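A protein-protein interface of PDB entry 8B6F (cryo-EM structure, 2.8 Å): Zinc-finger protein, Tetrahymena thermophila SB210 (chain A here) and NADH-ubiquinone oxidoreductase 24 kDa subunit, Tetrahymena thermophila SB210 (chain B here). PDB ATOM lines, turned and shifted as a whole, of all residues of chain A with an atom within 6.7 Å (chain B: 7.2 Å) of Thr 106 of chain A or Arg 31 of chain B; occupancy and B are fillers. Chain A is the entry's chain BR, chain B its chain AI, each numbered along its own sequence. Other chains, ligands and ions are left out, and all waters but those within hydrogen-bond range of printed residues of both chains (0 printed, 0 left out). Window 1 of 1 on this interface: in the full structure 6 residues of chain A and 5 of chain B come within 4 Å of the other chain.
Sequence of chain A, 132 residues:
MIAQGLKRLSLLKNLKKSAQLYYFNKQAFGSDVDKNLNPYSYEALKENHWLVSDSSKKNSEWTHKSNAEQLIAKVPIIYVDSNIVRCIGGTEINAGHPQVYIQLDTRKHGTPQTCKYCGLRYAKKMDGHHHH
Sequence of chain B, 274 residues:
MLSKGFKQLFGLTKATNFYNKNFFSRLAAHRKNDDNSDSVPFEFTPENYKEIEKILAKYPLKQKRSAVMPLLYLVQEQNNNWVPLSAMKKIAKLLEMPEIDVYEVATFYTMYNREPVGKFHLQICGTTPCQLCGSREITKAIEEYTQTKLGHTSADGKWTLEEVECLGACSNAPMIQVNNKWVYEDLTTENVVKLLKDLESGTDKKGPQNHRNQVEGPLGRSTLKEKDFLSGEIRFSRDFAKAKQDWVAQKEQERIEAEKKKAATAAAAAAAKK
Of the 13 printed residues of chain A, 6 touch a printed residue of chain B. Printed residues of chain A that touch a printed residue of chain B: Asn 83, Asp 105, Thr 106, Arg 107, Lys 108 and His 109. Hydrophobic or aromatic side chains of chain B within 4 Å of the printed part of chain A: Leu 27. Among the printed residues, Asp or Glu carboxylates within 4 Å of a Lys or Arg side-chain nitrogen of the other chain: Asp 105 of chain A with Arg 31 of chain B.
O of Asn 83 of chain A lies close to OE1 of Gln 103 of chain A, 2.8 Å away. The backbone carbonyl oxygen (O) of Lys 108 of chain A sits at hydrogen-bond distance from the side-chain hydroxyl (OG1) of Thr 111 of chain A (2.9 Å). The side-chain hydroxyl (OG1) of Thr 106 of chain A lies within hydrogen-bond range of the backbone carbonyl oxygen (O) of Thr 111 of chain A, at 3.4 Å. The backbone carbonyl oxygen (O) of Asn 83 of chain A lies within hydrogen-bond range of the backbone NH (N) of Asp 105 of chain A (3.4 Å). N of Asp 105 of chain A sits at hydrogen-bond distance from OE1 of Gln 103 of chain A, at 3.0 Å. The backbone carbonyl oxygen (O) of Asn 83 of chain A lies within hydrogen-bond range of the backbone NH (N) of Leu 104 of chain A, 2.5 Å away.
Of chain B, only Arg 31 (2.7 Å) comes within 4 Å of Thr 106 of chain A. Arg 31 of chain B touches just these residues of chain A: Asp 105 (3.7 Å), Thr 106 (2.7 Å), Arg 107 (3.1 Å) and His 109 (3.5 Å). Of the printed residues of chain A, His 30 of chain B touches Arg 107. Of the printed residues of chain B, His 109 of chain A touches Arg 31 (3.5 Å). The nearest residue of chain B that does not touch Thr 106 of chain A is Leu 27 of chain B (4.8 Å).
Among the printed residues, pairs that only touch across the chains: Asp 105 of chain A with Leu 27 of chain B, Arg 107 of chain A with Leu 27 of chain B, Arg 107 of chain A with His 30 of chain B, Arg 107 of chain A with Arg 31 of chain B, Lys 108 of chain A with Lys 32 of chain B and His 109 of chain A with Arg 31 of chain B.
NH1 of Arg 31 of chain B is in hydrogen-bond range of O of Thr 106 of chain A. The guanidinium group of Arg 26 of chain B sits close to the side-chain amide nitrogen of Asn 83 of chain A. The guanidinium group (NH2) of Arg 31 of chain B is in salt-bridge range of the side-chain carboxylate (OD1) of Asp 105 of chain A, at 3.7 Å. The backbone NH of Lys 32 of chain B lies within hydrogen-bond range of the backbone carbonyl oxygen of Arg 107 of chain A (2.9 Å).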
ATOM      1  N   ASN A  83       5.857  -8.034  -9.482  1.00  0.00           N
ATOM      2  CA  ASN A  83       5.393  -8.751  -8.300  1.00  0.00           C
ATOM      3  C   ASN A  83       5.542  -7.914  -7.037  1.00  0.00           C
ATOM      4  O   ASN A  83       4.821  -8.141  -6.060  1.00  0.00           O
ATOM      5  CB  ASN A  83       6.160 -10.064  -8.139  1.00  0.00           C
ATOM      6  CG  ASN A  83       5.843 -11.062  -9.231  1.00  0.00           C
ATOM      7  OD1 ASN A  83       4.741 -11.073  -9.778  1.00  0.00           O
ATOM      8  ND2 ASN A  83       6.808 -11.917  -9.550  1.00  0.00           N
ATOM      9  N   GLN A 103       4.328  -6.654  -1.472  1.00  0.00           N
ATOM     10  CA  GLN A 103       4.382  -7.874  -2.268  1.00  0.00           C
ATOM     11  C   GLN A 103       3.037  -8.100  -2.947  1.00  0.00           C
ATOM     12  O   GLN A 103       2.026  -8.326  -2.273  1.00  0.00           O
ATOM     13  CB  GLN A 103       4.740  -9.070  -1.389  1.00  0.00           C
ATOM     14  CG  GLN A 103       4.845 -10.385  -2.144  1.00  0.00           C
ATOM     15  CD  GLN A 103       5.904 -10.351  -3.224  1.00  0.00           C
ATOM     16  OE1 GLN A 103       5.594 -10.300  -4.412  1.00  0.00           O
ATOM     17  NE2 GLN A 103       7.168 -10.378  -2.814  1.00  0.00           N
ATOM     18  N   LEU A 104       3.025  -8.044  -4.276  1.00  0.00           N
ATOM     19  CA  LEU A 104       1.824  -8.306  -5.056  1.00  0.00           C
ATOM     20  C   LEU A 104       1.709  -9.759  -5.494  1.00  0.00           C
ATOM     21  O   LEU A 104       0.719 -10.121  -6.138  1.00  0.00           O
ATOM     22  CB  LEU A 104       1.792  -7.398  -6.289  1.00  0.00           C
ATOM     23  CG  LEU A 104       1.961  -5.901  -6.021  1.00  0.00           C
ATOM     24  CD1 LEU A 104       1.824  -5.117  -7.310  1.00  0.00           C
ATOM     25  CD2 LEU A 104       0.964  -5.407  -4.988  1.00  0.00           C
ATOM     26  N   ASP A 105       2.689 -10.599  -5.163  1.00  0.00           N
ATOM     27  CA  ASP A 105       2.646 -12.023  -5.496  1.00  0.00           C
ATOM     28  C   ASP A 105       1.945 -12.773  -4.362  1.00  0.00           C
ATOM     29  O   ASP A 105       2.526 -13.584  -3.638  1.00  0.00           O
ATOM     30  CB  ASP A 105       4.052 -12.552  -5.743  1.00  0.00           C
ATOM     31  CG  ASP A 105       4.063 -14.013  -6.145  1.00  0.00           C
ATOM     32  OD1 ASP A 105       3.511 -14.342  -7.215  1.00  0.00           O
ATOM     33  OD2 ASP A 105       4.631 -14.833  -5.392  1.00  0.00           O
ATOM     34  N   THR A 106       0.655 -12.481  -4.225  1.00  0.00           N
ATOM     35  CA  THR A 106      -0.144 -13.058  -3.156  1.00  0.00           C
ATOM     36  C   THR A 106      -0.341 -14.554  -3.372  1.00  0.00           C
ATOM     37  O   THR A 106      -0.348 -15.046  -4.502  1.00  0.00           O
ATOM     38  CB  THR A 106      -1.503 -12.364  -3.089  1.00  0.00           C
ATOM     39  OG1 THR A 106      -1.326 -10.950  -3.242  1.00  0.00           O
ATOM     40  CG2 THR A 106      -2.178 -12.631  -1.759  1.00  0.00           C
ATOM     41  N   ARG A 107      -0.501 -15.284  -2.264  1.00  0.00           N
ATOM     42  CA  ARG A 107      -0.765 -16.715  -2.360  1.00  0.00           C
ATOM     43  C   ARG A 107      -2.065 -17.005  -3.098  1.00  0.00           C
ATOM     44  O   ARG A 107      -2.260 -18.131  -3.569  1.00  0.00           O
ATOM     45  CB  ARG A 107      -0.807 -17.341  -0.965  1.00  0.00           C
ATOM     46  CG  ARG A 107      -1.913 -16.806  -0.074  1.00  0.00           C
ATOM     47  CD  ARG A 107      -1.866 -17.451   1.301  1.00  0.00           C
ATOM     48  NE  ARG A 107      -0.634 -17.130   2.012  1.00  0.00           N
ATOM     49  CZ  ARG A 107      -0.469 -16.071   2.794  1.00  0.00           C
ATOM     50  NH1 ARG A 107      -1.442 -15.196   2.991  1.00  0.00           N
ATOM     51  NH2 ARG A 107       0.703 -15.887   3.394  1.00  0.00           N
ATOM     52  N   LYS A 108      -2.958 -16.024  -3.195  1.00  0.00           N
ATOM     53  CA  LYS A 108      -4.143 -16.103  -4.039  1.00  0.00           C
ATOM     54  C   LYS A 108      -4.025 -15.018  -5.098  1.00  0.00           C
ATOM     55  O   LYS A 108      -3.940 -13.832  -4.767  1.00  0.00           O
ATOM     56  CB  LYS A 108      -5.420 -15.935  -3.215  1.00  0.00           C
ATOM     57  CG  LYS A 108      -6.689 -16.303  -3.961  1.00  0.00           C
ATOM     58  CD  LYS A 108      -7.891 -16.319  -3.029  1.00  0.00           C
ATOM     59  CE  LYS A 108      -9.135 -16.821  -3.744  1.00  0.00           C
ATOM     60  NZ  LYS A 108     -10.305 -16.914  -2.826  1.00  0.00           N
ATOM     61  N   HIS A 109      -4.026 -15.423  -6.365  1.00  0.00           N
ATOM     62  CA  HIS A 109      -3.721 -14.494  -7.445  1.00  0.00           C
ATOM     63  C   HIS A 109      -4.698 -13.326  -7.462  1.00  0.00           C
ATOM     64  O   HIS A 109      -5.907 -13.500  -7.290  1.00  0.00           O
ATOM     65  CB  HIS A 109      -3.756 -15.220  -8.791  1.00  0.00           C
ATOM     66  CG  HIS A 109      -2.765 -16.335  -8.902  1.00  0.00           C
ATOM     67  ND1 HIS A 109      -3.077 -17.642  -8.594  1.00  0.00           N
ATOM     68  CD2 HIS A 109      -1.465 -16.338  -9.281  1.00  0.00           C
ATOM     69  CE1 HIS A 109      -2.013 -18.403  -8.781  1.00  0.00           C
ATOM     70  NE2 HIS A 109      -1.021 -17.636  -9.198  1.00  0.00           N
ATOM     71  N   GLY A 110      -4.160 -12.126  -7.671  1.00  0.00           N
ATOM     72  CA  GLY A 110      -4.975 -10.948  -7.886  1.00  0.00           C
ATOM     73  C   GLY A 110      -5.522 -10.290  -6.642  1.00  0.00           C
ATOM     74  O   GLY A 110      -6.346  -9.376  -6.762  1.00  0.00           O
ATOM     75  N   THR A 111      -5.098 -10.708  -5.458  1.00  0.00           N
ATOM     76  CA  THR A 111      -5.606 -10.113  -4.229  1.00  0.00           C
ATOM     77  C   THR A 111      -4.972  -8.741  -4.021  1.00  0.00           C
ATOM     78  O   THR A 111      -3.742  -8.649  -3.935  1.00  0.00           O
ATOM     79  CB  THR A 111      -5.304 -11.007  -3.035  1.00  0.00           C
ATOM     80  OG1 THR A 111      -5.843 -12.314  -3.265  1.00  0.00           O
ATOM     81  CG2 THR A 111      -5.912 -10.430  -1.762  1.00  0.00           C
ATOM     82  N   PRO A 112      -5.752  -7.666  -3.938  1.00  0.00           N
ATOM     83  CA  PRO A 112      -5.152  -6.349  -3.706  1.00  0.00           C
ATOM     84  C   PRO A 112      -4.539  -6.248  -2.320  1.00  0.00           C
ATOM     85  O   PRO A 112      -5.017  -6.847  -1.354  1.00  0.00           O
ATOM     86  CB  PRO A 112      -6.333  -5.385  -3.866  1.00  0.00           C
ATOM     87  CG  PRO A 112      -7.528  -6.202  -3.553  1.00  0.00           C
ATOM     88  CD  PRO A 112      -7.221  -7.590  -4.030  1.00  0.00           C
ATOM     89  N   GLN A 113      -3.463  -5.470  -2.235  1.00  0.00           N
ATOM     90  CA  GLN A 113      -2.771  -5.196  -0.984  1.00  0.00           C
ATOM     91  C   GLN A 113      -2.713  -3.691  -0.775  1.00  0.00           C
ATOM     92  O   GLN A 113      -2.370  -2.947  -1.700  1.00  0.00           O
ATOM     93  CB  GLN A 113      -1.358  -5.785  -0.995  1.00  0.00           C
ATOM     94  CG  GLN A 113      -1.314  -7.299  -1.141  1.00  0.00           C
ATOM     95  CD  GLN A 113      -1.897  -8.020   0.059  1.00  0.00           C
ATOM     96  OE1 GLN A 113      -2.252  -7.399   1.059  1.00  0.00           O
ATOM     97  NE2 GLN A 113      -1.993  -9.342  -0.034  1.00  0.00           N
ATOM     98  N   LYS A 124      -1.576  -7.081  -8.662  1.00  0.00           N
ATOM     99  CA  LYS A 124      -0.796  -7.522  -9.808  1.00  0.00           C
ATOM    100  C   LYS A 124      -1.694  -7.676 -11.027  1.00  0.00           C
ATOM    101  O   LYS A 124      -2.821  -8.169 -10.931  1.00  0.00           O
ATOM    102  CB  LYS A 124      -0.091  -8.842  -9.504  1.00  0.00           C
ATOM    103  CG  LYS A 124       0.802  -9.331 -10.636  1.00  0.00           C
ATOM    104  CD  LYS A 124       1.535 -10.606 -10.257  1.00  0.00           C
ATOM    105  CE  LYS A 124       2.369 -11.128 -11.414  1.00  0.00           C
ATOM    106  NZ  LYS A 124       1.546 -11.432 -12.617  1.00  0.00           N
ATOM    107  N   ARG B  26       7.767 -21.582  -6.961  1.00  0.00           N
ATOM    108  CA  ARG B  26       7.687 -20.129  -7.016  1.00  0.00           C
ATOM    109  C   ARG B  26       7.440 -19.500  -5.654  1.00  0.00           C
ATOM    110  O   ARG B  26       8.207 -18.633  -5.226  1.00  0.00           O
ATOM    111  CB  ARG B  26       6.573 -19.704  -7.985  1.00  0.00           C
ATOM    112  CG  ARG B  26       6.961 -19.757  -9.455  1.00  0.00           C
ATOM    113  CD  ARG B  26       7.955 -18.658  -9.816  1.00  0.00           C
ATOM    114  NE  ARG B  26       7.437 -17.328  -9.517  1.00  0.00           N
ATOM    115  CZ  ARG B  26       8.107 -16.200  -9.713  1.00  0.00           C
ATOM    116  NH1 ARG B  26       9.331 -16.200 -10.215  1.00  0.00           N
ATOM    117  NH2 ARG B  26       7.533 -15.042  -9.397  1.00  0.00           N
ATOM    118  N   LEU B  27       6.386 -19.915  -4.960  1.00  0.00           N
ATOM    119  CA  LEU B  27       6.017 -19.338  -3.678  1.00  0.00           C
ATOM    120  C   LEU B  27       6.464 -20.245  -2.541  1.00  0.00           C
ATOM    121  O   LEU B  27       6.556 -21.466  -2.693  1.00  0.00           O
ATOM    122  CB  LEU B  27       4.504 -19.116  -3.603  1.00  0.00           C
ATOM    123  CG  LEU B  27       3.978 -18.376  -2.371  1.00  0.00           C
ATOM    124  CD1 LEU B  27       4.521 -16.956  -2.312  1.00  0.00           C
ATOM    125  CD2 LEU B  27       2.459 -18.369  -2.365  1.00  0.00           C
ATOM    126  N   ALA B  28       6.743 -19.633  -1.389  1.00  0.00           N
ATOM    127  CA  ALA B  28       7.139 -20.360  -0.189  1.00  0.00           C
ATOM    128  C   ALA B  28       5.954 -20.687   0.709  1.00  0.00           C
ATOM    129  O   ALA B  28       6.117 -20.810   1.930  1.00  0.00           O
ATOM    130  CB  ALA B  28       8.187 -19.559   0.585  1.00  0.00           C
ATOM    131  N   ALA B  29       4.762 -20.825   0.133  1.00  0.00           N
ATOM    132  CA  ALA B  29       3.561 -21.136   0.889  1.00  0.00           C
ATOM    133  C   ALA B  29       2.578 -21.830  -0.043  1.00  0.00           C
ATOM    134  O   ALA B  29       2.840 -22.002  -1.236  1.00  0.00           O
ATOM    135  CB  ALA B  29       2.952 -19.872   1.506  1.00  0.00           C
ATOM    136  N   HIS B  30       1.439 -22.232   0.510  1.00  0.00           N
ATOM    137  CA  HIS B  30       0.436 -22.943  -0.272  1.00  0.00           C
ATOM    138  C   HIS B  30      -0.284 -21.971  -1.195  1.00  0.00           C
ATOM    139  O   HIS B  30      -0.894 -21.001  -0.732  1.00  0.00           O
ATOM    140  CB  HIS B  30      -0.560 -23.642   0.649  1.00  0.00           C
ATOM    141  CG  HIS B  30      -1.604 -24.422  -0.082  1.00  0.00           C
ATOM    142  ND1 HIS B  30      -2.931 -24.049  -0.110  1.00  0.00           N
ATOM    143  CD2 HIS B  30      -1.517 -25.551  -0.824  1.00  0.00           C
ATOM    144  CE1 HIS B  30      -3.616 -24.916  -0.833  1.00  0.00           C
ATOM    145  NE2 HIS B  30      -2.782 -25.838  -1.278  1.00  0.00           N
ATOM    146  N   ARG B  31      -0.218 -22.229  -2.497  1.00  0.00           N
ATOM    147  CA  ARG B  31      -0.945 -21.422  -3.465  1.00  0.00           C
ATOM    148  C   ARG B  31      -2.410 -21.837  -3.470  1.00  0.00           C
ATOM    149  O   ARG B  31      -2.726 -23.029  -3.523  1.00  0.00           O
ATOM    150  CB  ARG B  31      -0.342 -21.586  -4.859  1.00  0.00           C
ATOM    151  CG  ARG B  31      -0.936 -20.658  -5.908  1.00  0.00           C
ATOM    152  CD  ARG B  31      -0.425 -19.235  -5.757  1.00  0.00           C
ATOM    153  NE  ARG B  31       0.936 -19.087  -6.259  1.00  0.00           N
ATOM    154  CZ  ARG B  31       1.556 -17.925  -6.410  1.00  0.00           C
ATOM    155  NH1 ARG B  31       0.963 -16.780  -6.112  1.00  0.00           N
ATOM    156  NH2 ARG B  31       2.802 -17.910  -6.874  1.00  0.00           N
ATOM    157  N   LYS B  32      -3.302 -20.850  -3.421  1.00  0.00           N
ATOM    158  CA  LYS B  32      -4.733 -21.121  -3.372  1.00  0.00           C
ATOM    159  C   LYS B  32      -5.224 -21.603  -4.730  1.00  0.00           C
ATOM    160  O   LYS B  32      -5.539 -20.792  -5.607  1.00  0.00           O
ATOM    161  CB  LYS B  32      -5.496 -19.868  -2.938  1.00  0.00           C
ATOM    162  CG  LYS B  32      -6.995 -20.066  -2.768  1.00  0.00           C
ATOM    163  CD  LYS B  32      -7.306 -21.045  -1.648  1.00  0.00           C
ATOM    164  CE  LYS B  32      -8.802 -21.114  -1.377  1.00  0.00           C
ATOM    165  NZ  LYS B  32      -9.573 -21.542  -2.579  1.00  0.00           N
ATOM    166  N   ASN B  33      -5.290 -22.919  -4.910  1.00  0.00           N
ATOM    167  CA  ASN B  33      -5.724 -23.530  -6.156  1.00  0.00           C
ATOM    168  C   ASN B  33      -6.902 -24.453  -5.886  1.00  0.00           C
ATOM    169  O   ASN B  33      -6.944 -25.137  -4.859  1.00  0.00           O
ATOM    170  CB  ASN B  33      -4.584 -24.313  -6.812  1.00  0.00           C
ATOM    171  CG  ASN B  33      -4.983 -24.920  -8.140  1.00  0.00           C
ATOM    172  OD1 ASN B  33      -6.014 -24.567  -8.713  1.00  0.00           O
ATOM    173  ND2 ASN B  33      -4.164 -25.838  -8.640  1.00  0.00           N
ATOM    174  N   ASP B  34      -7.864 -24.464  -6.811  1.00  0.00           N
ATOM    175  CA  ASP B  34      -9.047 -25.298  -6.631  1.00  0.00           C
ATOM    176  C   ASP B  34      -8.730 -26.774  -6.820  1.00  0.00           C
ATOM    177  O   ASP B  34      -9.408 -27.630  -6.241  1.00  0.00           O
ATOM    178  CB  ASP B  34     -10.144 -24.868  -7.606  1.00  0.00           C
ATOM    179  CG  ASP B  34     -10.524 -23.409  -7.447  1.00  0.00           C
ATOM    180  OD1 ASP B  34      -9.891 -22.715  -6.624  1.00  0.00           O
ATOM    181  OD2 ASP B  34     -11.457 -22.957  -8.145  1.00  0.00           O
ATOM    182  N   ASN B  36      -5.899 -28.190  -5.911  1.00  0.00           N
ATOM    183  CA  ASN B  36      -4.954 -28.614  -4.886  1.00  0.00           C
ATOM    184  C   ASN B  36      -5.518 -28.355  -3.495  1.00  0.00           C
ATOM    185  O   ASN B  36      -4.767 -28.169  -2.535  1.00  0.00           O
ATOM    186  CB  ASN B  36      -3.610 -27.907  -5.061  1.00  0.00           C
ATOM    187  CG  ASN B  36      -2.517 -28.519  -4.213  1.00  0.00           C
ATOM    188  OD1 ASN B  36      -2.606 -29.677  -3.809  1.00  0.00           O
ATOM    189  ND2 ASN B  36      -1.476 -27.744  -3.938  1.00  0.00           N
ATOM    190  N   SER B  37      -6.842 -28.339  -3.372  1.00  0.00           N
ATOM    191  CA  SER B  37      -7.472 -28.113  -2.084  1.00  0.00           C
ATOM    192  C   SER B  37      -7.290 -29.334  -1.185  1.00  0.00           C
ATOM    193  O   SER B  37      -6.865 -30.408  -1.619  1.00  0.00           O
ATOM    194  CB  SER B  37      -8.957 -27.795  -2.259  1.00  0.00           C
ATOM    195  OG  SER B  37      -9.639 -28.864  -2.893  1.00  0.00           O
ATOM    196  N   ARG B 114       5.449 -28.607  -6.318  1.00  0.00           N
ATOM    197  CA  ARG B 114       4.266 -28.484  -5.480  1.00  0.00           C
ATOM    198  C   ARG B 114       3.008 -28.164  -6.275  1.00  0.00           C
ATOM    199  O   ARG B 114       1.914 -28.185  -5.703  1.00  0.00           O
ATOM    200  CB  ARG B 114       4.488 -27.410  -4.412  1.00  0.00           C
ATOM    201  CG  ARG B 114       5.510 -27.811  -3.357  1.00  0.00           C
ATOM    202  CD  ARG B 114       5.675 -26.747  -2.284  1.00  0.00           C
ATOM    203  NE  ARG B 114       6.336 -25.547  -2.783  1.00  0.00           N
ATOM    204  CZ  ARG B 114       5.710 -24.483  -3.271  1.00  0.00           C
ATOM    205  NH1 ARG B 114       4.391 -24.432  -3.354  1.00  0.00           N
ATOM    206  NH2 ARG B 114       6.428 -23.444  -3.685  1.00  0.00           N
ATOM    207  N   GLU B 115       3.132 -27.878  -7.564  1.00  0.00           N
ATOM    208  CA  GLU B 115       2.008 -27.607  -8.444  1.00  0.00           C
ATOM    209  C   GLU B 115       2.151 -28.425  -9.716  1.00  0.00           C
ATOM    210  O   GLU B 115       3.259 -28.834 -10.080  1.00  0.00           O
ATOM    211  CB  GLU B 115       1.917 -26.115  -8.793  1.00  0.00           C
ATOM    212  CG  GLU B 115       1.535 -25.234  -7.616  1.00  0.00           C
ATOM    213  CD  GLU B 115       1.409 -23.774  -8.000  1.00  0.00           C
ATOM    214  OE1 GLU B 115       1.872 -23.406  -9.099  1.00  0.00           O
ATOM    215  OE2 GLU B 115       0.845 -22.996  -7.204  1.00  0.00           O
